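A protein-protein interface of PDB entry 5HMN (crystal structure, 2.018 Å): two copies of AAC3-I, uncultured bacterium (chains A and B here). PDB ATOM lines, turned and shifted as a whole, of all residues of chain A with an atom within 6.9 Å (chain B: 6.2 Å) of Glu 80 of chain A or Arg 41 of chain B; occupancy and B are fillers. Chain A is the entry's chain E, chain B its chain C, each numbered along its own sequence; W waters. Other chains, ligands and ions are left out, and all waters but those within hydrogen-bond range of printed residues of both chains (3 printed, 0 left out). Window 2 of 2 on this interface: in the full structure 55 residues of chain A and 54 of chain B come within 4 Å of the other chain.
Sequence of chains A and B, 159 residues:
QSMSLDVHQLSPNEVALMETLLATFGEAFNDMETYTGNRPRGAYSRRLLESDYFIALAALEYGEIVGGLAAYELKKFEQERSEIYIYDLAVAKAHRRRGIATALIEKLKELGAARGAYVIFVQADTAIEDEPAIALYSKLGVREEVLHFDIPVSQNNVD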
ATOM      1  N   LYS A  76     -24.042  26.840 -23.248  1.00  0.00           N
ATOM      2  CA  LYS A  76     -23.752  26.747 -21.821  1.00  0.00           C
ATOM      3  C   LYS A  76     -22.386  26.124 -21.560  1.00  0.00           C
ATOM      4  O   LYS A  76     -21.849  25.383 -22.385  1.00  0.00           O
ATOM      5  CB  LYS A  76     -24.846  25.954 -21.100  1.00  0.00           C
ATOM      6  CG  LYS A  76     -26.222  26.618 -21.148  1.00  0.00           C
ATOM      7  CD  LYS A  76     -26.145  28.119 -20.837  1.00  0.00           C
ATOM      8  CE  LYS A  76     -25.708  28.392 -19.402  1.00  0.00           C
ATOM      9  NZ  LYS A  76     -26.620  27.770 -18.408  1.00  0.00           N
ATOM     10  N   PHE A  77     -21.832  26.438 -20.397  1.00  0.00           N
ATOM     11  CA  PHE A  77     -20.476  26.038 -20.044  1.00  0.00           C
ATOM     12  C   PHE A  77     -20.459  24.876 -19.061  1.00  0.00           C
ATOM     13  O   PHE A  77     -19.474  24.137 -18.980  1.00  0.00           O
ATOM     14  CB  PHE A  77     -19.725  27.238 -19.458  1.00  0.00           C
ATOM     15  CG  PHE A  77     -20.538  28.031 -18.462  1.00  0.00           C
ATOM     16  CD1 PHE A  77     -21.378  29.056 -18.882  1.00  0.00           C
ATOM     17  CD2 PHE A  77     -20.474  27.738 -17.112  1.00  0.00           C
ATOM     18  CE1 PHE A  77     -22.132  29.774 -17.971  1.00  0.00           C
ATOM     19  CE2 PHE A  77     -21.221  28.454 -16.194  1.00  0.00           C
ATOM     20  CZ  PHE A  77     -22.052  29.473 -16.624  1.00  0.00           C
ATOM     21  N   GLU A  78     -21.549  24.714 -18.314  1.00  0.00           N
ATOM     22  CA  GLU A  78     -21.624  23.655 -17.309  1.00  0.00           C
ATOM     23  C   GLU A  78     -21.964  22.312 -17.957  1.00  0.00           C
ATOM     24  O   GLU A  78     -21.612  21.260 -17.434  1.00  0.00           O
ATOM     25  CB  GLU A  78     -22.656  24.000 -16.228  1.00  0.00           C
ATOM     26  CG  GLU A  78     -24.111  23.936 -16.673  1.00  0.00           C
ATOM     27  CD  GLU A  78     -24.531  25.113 -17.541  1.00  0.00           C
ATOM     28  OE1 GLU A  78     -23.747  26.077 -17.683  1.00  0.00           O
ATOM     29  OE2 GLU A  78     -25.653  25.071 -18.084  1.00  0.00           O
ATOM     30  N   GLN A  79     -22.645  22.368 -19.094  1.00  0.00           N
ATOM     31  CA  GLN A  79     -23.037  21.175 -19.850  1.00  0.00           C
ATOM     32  C   GLN A  79     -23.046  21.484 -21.342  1.00  0.00           C
ATOM     33  O   GLN A  79     -23.086  22.649 -21.740  1.00  0.00           O
ATOM     34  CB  GLN A  79     -24.420  20.671 -19.419  1.00  0.00           C
ATOM     35  CG  GLN A  79     -24.497  20.134 -17.999  1.00  0.00           C
ATOM     36  CD  GLN A  79     -25.892  19.680 -17.622  1.00  0.00           C
ATOM     37  OE1 GLN A  79     -26.656  19.215 -18.467  1.00  0.00           O
ATOM     38  NE2 GLN A  79     -26.233  19.820 -16.346  1.00  0.00           N
ATOM     39  N   GLU A  80     -23.016  20.443 -22.168  1.00  0.00           N
ATOM     40  CA  GLU A  80     -23.109  20.625 -23.611  1.00  0.00           C
ATOM     41  C   GLU A  80     -24.554  20.855 -24.023  1.00  0.00           C
ATOM     42  O   GLU A  80     -25.161  20.013 -24.678  1.00  0.00           O
ATOM     43  CB  GLU A  80     -22.537  19.417 -24.353  1.00  0.00           C
ATOM     44  CG  GLU A  80     -21.040  19.255 -24.195  1.00  0.00           C
ATOM     45  CD  GLU A  80     -20.486  18.136 -25.047  1.00  0.00           C
ATOM     46  OE1 GLU A  80     -20.738  18.136 -26.271  1.00  0.00           O
ATOM     47  OE2 GLU A  80     -19.802  17.253 -24.492  1.00  0.00           O
ATOM     48  N   ARG A  81     -25.097  22.000 -23.622  1.00  0.00           N
ATOM     49  CA  ARG A  81     -26.468  22.371 -23.942  1.00  0.00           C
ATOM     50  C   ARG A  81     -26.524  23.853 -24.271  1.00  0.00           C
ATOM     51  O   ARG A  81     -25.572  24.586 -24.005  1.00  0.00           O
ATOM     52  CB  ARG A  81     -27.405  22.042 -22.779  1.00  0.00           C
ATOM     53  CG  ARG A  81     -27.040  22.739 -21.471  1.00  0.00           C
ATOM     54  CD  ARG A  81     -27.904  22.251 -20.318  1.00  0.00           C
ATOM     55  NE  ARG A  81     -27.684  23.032 -19.100  1.00  0.00           N
ATOM     56  CZ  ARG A  81     -28.388  22.887 -17.982  1.00  0.00           C
ATOM     57  NH1 ARG A  81     -29.359  21.983 -17.919  1.00  0.00           N
ATOM     58  NH2 ARG A  81     -28.124  23.645 -16.926  1.00  0.00           N
ATOM     59  N   SER A  82     -27.636  24.300 -24.842  1.00  0.00           N
ATOM     60  CA  SER A  82     -27.773  25.705 -25.215  1.00  0.00           C
ATOM     61  C   SER A  82     -29.049  26.325 -24.663  1.00  0.00           C
ATOM     62  O   SER A  82     -30.004  25.625 -24.331  1.00  0.00           O
ATOM     63  CB  SER A  82     -27.739  25.860 -26.736  1.00  0.00           C
ATOM     64  OG  SER A  82     -26.452  25.558 -27.246  1.00  0.00           O
ATOM     65  N   ARG A 115     -30.252  22.651 -32.166  1.00  0.00           N
ATOM     66  CA  ARG A 115     -29.039  23.271 -31.644  1.00  0.00           C
ATOM     67  C   ARG A 115     -28.713  22.734 -30.258  1.00  0.00           C
ATOM     68  O   ARG A 115     -27.712  23.120 -29.652  1.00  0.00           O
ATOM     69  CB  ARG A 115     -29.187  24.793 -31.592  1.00  0.00           C
ATOM     70  CG  ARG A 115     -29.224  25.474 -32.950  1.00  0.00           C
ATOM     71  CD  ARG A 115     -29.603  26.942 -32.812  1.00  0.00           C
ATOM     72  NE  ARG A 115     -29.542  27.649 -34.088  1.00  0.00           N
ATOM     73  CZ  ARG A 115     -28.604  28.534 -34.406  1.00  0.00           C
ATOM     74  NH1 ARG A 115     -27.651  28.835 -33.537  1.00  0.00           N
ATOM     75  NH2 ARG A 115     -28.626  29.128 -35.591  1.00  0.00           N
ATOM     76  N   GLY A 116     -29.567  21.846 -29.756  1.00  0.00           N
ATOM     77  CA  GLY A 116     -29.378  21.277 -28.434  1.00  0.00           C
ATOM     78  C   GLY A 116     -29.891  22.188 -27.336  1.00  0.00           C
ATOM     79  O   GLY A 116     -29.526  22.040 -26.169  1.00  0.00           O
ATOM     80  N   VAL B  15      -8.942  25.100 -19.884  1.00  0.00           N
ATOM     81  CA  VAL B  15     -10.179  24.355 -19.667  1.00  0.00           C
ATOM     82  C   VAL B  15     -10.189  23.740 -18.267  1.00  0.00           C
ATOM     83  O   VAL B  15     -11.238  23.646 -17.623  1.00  0.00           O
ATOM     84  CB  VAL B  15     -10.365  23.246 -20.727  1.00  0.00           C
ATOM     85  CG1 VAL B  15     -11.570  22.375 -20.400  1.00  0.00           C
ATOM     86  CG2 VAL B  15     -10.509  23.858 -22.114  1.00  0.00           C
ATOM     87  N   ASN B  38     -22.516  16.564 -15.162  1.00  0.00           N
ATOM     88  CA  ASN B  38     -22.388  16.186 -16.563  1.00  0.00           C
ATOM     89  C   ASN B  38     -21.540  17.193 -17.328  1.00  0.00           C
ATOM     90  O   ASN B  38     -22.017  17.838 -18.262  1.00  0.00           O
ATOM     91  CB  ASN B  38     -23.766  16.052 -17.212  1.00  0.00           C
ATOM     92  CG  ASN B  38     -23.736  15.220 -18.481  1.00  0.00           C
ATOM     93  OD1 ASN B  38     -22.703  15.105 -19.144  1.00  0.00           O
ATOM     94  ND2 ASN B  38     -24.875  14.631 -18.826  1.00  0.00           N
ATOM     95  N   ARG B  39     -20.282  17.317 -16.919  1.00  0.00           N
ATOM     96  CA  ARG B  39     -19.353  18.279 -17.505  1.00  0.00           C
ATOM     97  C   ARG B  39     -19.118  18.008 -18.989  1.00  0.00           C
ATOM     98  O   ARG B  39     -19.101  16.855 -19.420  1.00  0.00           O
ATOM     99  CB  ARG B  39     -18.020  18.251 -16.753  1.00  0.00           C
ATOM    100  CG  ARG B  39     -18.156  18.296 -15.239  1.00  0.00           C
ATOM    101  CD  ARG B  39     -16.817  18.062 -14.564  1.00  0.00           C
ATOM    102  NE  ARG B  39     -16.908  18.163 -13.112  1.00  0.00           N
ATOM    103  CZ  ARG B  39     -16.144  17.479 -12.268  1.00  0.00           C
ATOM    104  NH1 ARG B  39     -15.230  16.637 -12.734  1.00  0.00           N
ATOM    105  NH2 ARG B  39     -16.294  17.631 -10.959  1.00  0.00           N
ATOM    106  N   PRO B  40     -18.944  19.077 -19.778  1.00  0.00           N
ATOM    107  CA  PRO B  40     -18.662  18.968 -21.213  1.00  0.00           C
ATOM    108  C   PRO B  40     -17.298  18.354 -21.494  1.00  0.00           C
ATOM    109  O   PRO B  40     -16.490  18.221 -20.579  1.00  0.00           O
ATOM    110  CB  PRO B  40     -18.695  20.423 -21.691  1.00  0.00           C
ATOM    111  CG  PRO B  40     -19.453  21.166 -20.645  1.00  0.00           C
ATOM    112  CD  PRO B  40     -19.106  20.479 -19.359  1.00  0.00           C
ATOM    113  N   ARG B  41     -17.046  17.989 -22.748  1.00  0.00           N
ATOM    114  CA  ARG B  41     -15.727  17.513 -23.145  1.00  0.00           C
ATOM    115  C   ARG B  41     -14.780  18.693 -23.254  1.00  0.00           C
ATOM    116  O   ARG B  41     -15.223  19.827 -23.415  1.00  0.00           O
ATOM    117  CB  ARG B  41     -15.794  16.768 -24.474  1.00  0.00           C
ATOM    118  CG  ARG B  41     -16.974  15.837 -24.592  1.00  0.00           C
ATOM    119  CD  ARG B  41     -17.376  15.672 -26.045  1.00  0.00           C
ATOM    120  NE  ARG B  41     -18.616  14.919 -26.186  1.00  0.00           N
ATOM    121  CZ  ARG B  41     -19.151  14.575 -27.352  1.00  0.00           C
ATOM    122  NH1 ARG B  41     -18.553  14.917 -28.487  1.00  0.00           N
ATOM    123  NH2 ARG B  41     -20.283  13.886 -27.385  1.00  0.00           N
ATOM    124  N   GLY B  42     -13.480  18.425 -23.173  1.00  0.00           N
ATOM    125  CA  GLY B  42     -12.479  19.472 -23.266  1.00  0.00           C
ATOM    126  C   GLY B  42     -12.567  20.225 -24.577  1.00  0.00           C
ATOM    127  O   GLY B  42     -12.311  21.428 -24.628  1.00  0.00           O
ATOM    128  N   ALA B  43     -12.940  19.513 -25.638  1.00  0.00           N
ATOM    129  CA  ALA B  43     -13.068  20.110 -26.959  1.00  0.00           C
ATOM    130  C   ALA B  43     -14.191  21.140 -26.989  1.00  0.00           C
ATOM    131  O   ALA B  43     -14.012  22.245 -27.500  1.00  0.00           O
ATOM    132  CB  ALA B  43     -13.307  19.031 -28.007  1.00  0.00           C
ATOM    133  N   TYR B  44     -15.345  20.770 -26.442  1.00  0.00           N
ATOM    134  CA  TYR B  44     -16.495  21.670 -26.375  1.00  0.00           C
ATOM    135  C   TYR B  44     -16.176  22.896 -25.529  1.00  0.00           C
ATOM    136  O   TYR B  44     -16.438  24.033 -25.931  1.00  0.00           O
ATOM    137  CB  TYR B  44     -17.717  20.936 -25.810  1.00  0.00           C
ATOM    138  CG  TYR B  44     -18.934  21.816 -25.575  1.00  0.00           C
ATOM    139  CD1 TYR B  44     -19.116  22.477 -24.368  1.00  0.00           C
ATOM    140  CD2 TYR B  44     -19.902  21.975 -26.558  1.00  0.00           C
ATOM    141  CE1 TYR B  44     -20.216  23.273 -24.148  1.00  0.00           C
ATOM    142  CE2 TYR B  44     -21.012  22.770 -26.346  1.00  0.00           C
ATOM    143  CZ  TYR B  44     -21.162  23.416 -25.138  1.00  0.00           C
ATOM    144  OH  TYR B  44     -22.257  24.215 -24.900  1.00  0.00           O
ATOM    145  N   SER B  45     -15.609  22.659 -24.351  1.00  0.00           N
ATOM    146  CA  SER B  45     -15.257  23.744 -23.443  1.00  0.00           C
ATOM    147  C   SER B  45     -14.222  24.662 -24.078  1.00  0.00           C
ATOM    148  O   SER B  45     -14.256  25.872 -23.901  1.00  0.00           O
ATOM    149  CB  SER B  45     -14.727  23.187 -22.118  1.00  0.00           C
ATOM    150  OG  SER B  45     -15.694  22.368 -21.488  1.00  0.00           O
ATOM    151  N   ARG B  46     -13.302  24.084 -24.841  1.00  0.00           N
ATOM    152  CA  ARG B  46     -12.264  24.892 -25.462  1.00  0.00           C
ATOM    153  C   ARG B  46     -12.792  25.841 -26.538  1.00  0.00           C
ATOM    154  O   ARG B  46     -12.454  27.026 -26.556  1.00  0.00           O
ATOM    155  CB  ARG B  46     -11.199  24.010 -26.078  1.00  0.00           C
ATOM    156  CG  ARG B  46     -10.171  24.833 -26.788  1.00  0.00           C
ATOM    157  CD  ARG B  46      -9.031  23.989 -27.298  1.00  0.00           C
ATOM    158  NE  ARG B  46      -7.817  24.787 -27.447  1.00  0.00           N
ATOM    159  CZ  ARG B  46      -7.636  25.703 -28.387  1.00  0.00           C
ATOM    160  NH1 ARG B  46      -8.585  25.954 -29.282  1.00  0.00           N
ATOM    161  NH2 ARG B  46      -6.497  26.378 -28.439  1.00  0.00           N
HETATM  162  O   HOH W   1     -22.557  19.232 -15.079  1.00  0.00           O
HETATM  163  O   HOH W   2     -22.039  17.900 -20.887  1.00  0.00           O
HETATM  164  O   HOH W   3     -24.031  24.266 -26.880  1.00  0.00           O
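The side-chain carboxylate of Glu 80 of chain A lies within salt-bridge range of the guanidinium group of Arg 41 of chain B (3.1 Å).
OH of Tyr 44 of chain B lies within hydrogen-bond range of O of Lys 76 of chain A (2.8 Å).
The side-chain hydroxyl (OH) of Tyr 44 of chain B is in hydrogen-bond range of the backbone carbonyl oxygen (O) of Arg 81 of chain A (3.5 Å).
The backbone carbonyl oxygen (O) of Arg 41 of chain B sits at hydrogen-bond distance from the side-chain hydroxyl (OG) of Ser 45 of chain B (3.2 Å).
The side-chain amino group of Lys 76 of chain A is in salt-bridge range of the side-chain carboxylate of Glu 78 of chain A (2.9 Å).
N of Lys 76 of chain A is in hydrogen-bond range of O of Arg 81 of chain A (2.8 Å).
OE2 of Glu 78 of chain A lies within salt-bridge range of NE of Arg 81 of chain A, at 3.1 Å.
CG of Pro 40 of chain B touches O of Phe 77 of chain A, 3.4 Å away.
O of Glu 78 of chain A touches O of Asn 38 of chain B (3.5 Å).
CA of Arg 39 of chain B touches O of Glu 78 of chain A, 3.7 Å away.
O of Glu 78 of chain A touches CD of Pro 40 of chain B, at 3.3 Å.
Gln 79 of chain A touches Asn 38 of chain B (CG to O, 3.4 Å).
Gln 79 of chain A touches Pro 40 of chain B (CA to CG, 3.7 Å).
O of Gln 79 of chain A touches OH of Tyr 44 of chain B (3.6 Å).
CG of Glu 80 of chain A touches CB of Pro 40 of chain B, 3.6 Å away.
Glu 80 of chain A touches Tyr 44 of chain B (CG to CG, 3.6 Å).
Glu 80 of chain A touches just these residues of chain B: Pro 40, Arg 41 and Tyr 44.
Printed residues of chain A within 4 Å of Arg 41 of chain B: Glu 80 (3.1 Å).
Printed residues of chain B within 4 Å of Arg 81 of chain A: Tyr 44 (3.5 Å).
Of the printed residues of chain B, Lys 76 of chain A touches Tyr 44.
Of the printed residues of chain B, Gln 79 of chain A touches Asn 38 (3.4 Å), Pro 40 (3.7 Å) and Tyr 44 (3.6 Å).
Of the printed residues of chain B, Phe 77 of chain A touches Pro 40.
Of the printed residues of chain A, Arg 39 of chain B touches Glu 78 (3.7 Å).
The nearest printed residue of chain A that does not touch Asn 38 of chain B is Glu 80 of chain A (4.8 Å).
Of the 10 printed residues of chain B, 5 touch a printed residue of chain A.
Printed residues of chain A that touch a printed residue of chain B: Lys 76, Phe 77, Glu 78, Gln 79, Glu 80 and Arg 81.
Among the printed residues, Asp or Glu carboxylates within 4 Å of a Lys or Arg side-chain nitrogen of the other chain: Glu 80 of chain A with Arg 41 of chain B.
No position is printed for both chains.
Water W2 lies within hydrogen-bond range of the backbone carbonyl oxygen (O) of Asn 38 of chain B (2.6 Å), the backbone NH (N) of Glu 80 of chain A (3.0 Å) and the backbone carbonyl oxygen (O) of Arg 39 of chain B (3.4 Å).
Water W3 lies within hydrogen-bond range of the side-chain hydroxyl (OH) of Tyr 44 of chain B (2.7 Å), the side-chain hydroxyl (OG) of Ser 82 of chain A (2.8 Å) and the backbone carbonyl oxygen (O) of Arg 81 of chain A (3.3 Å).
Water W1 lies within hydrogen-bond range of N of Asn 38 of chain B, O of Glu 78 of chain A and N of Arg 39 of chain B.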
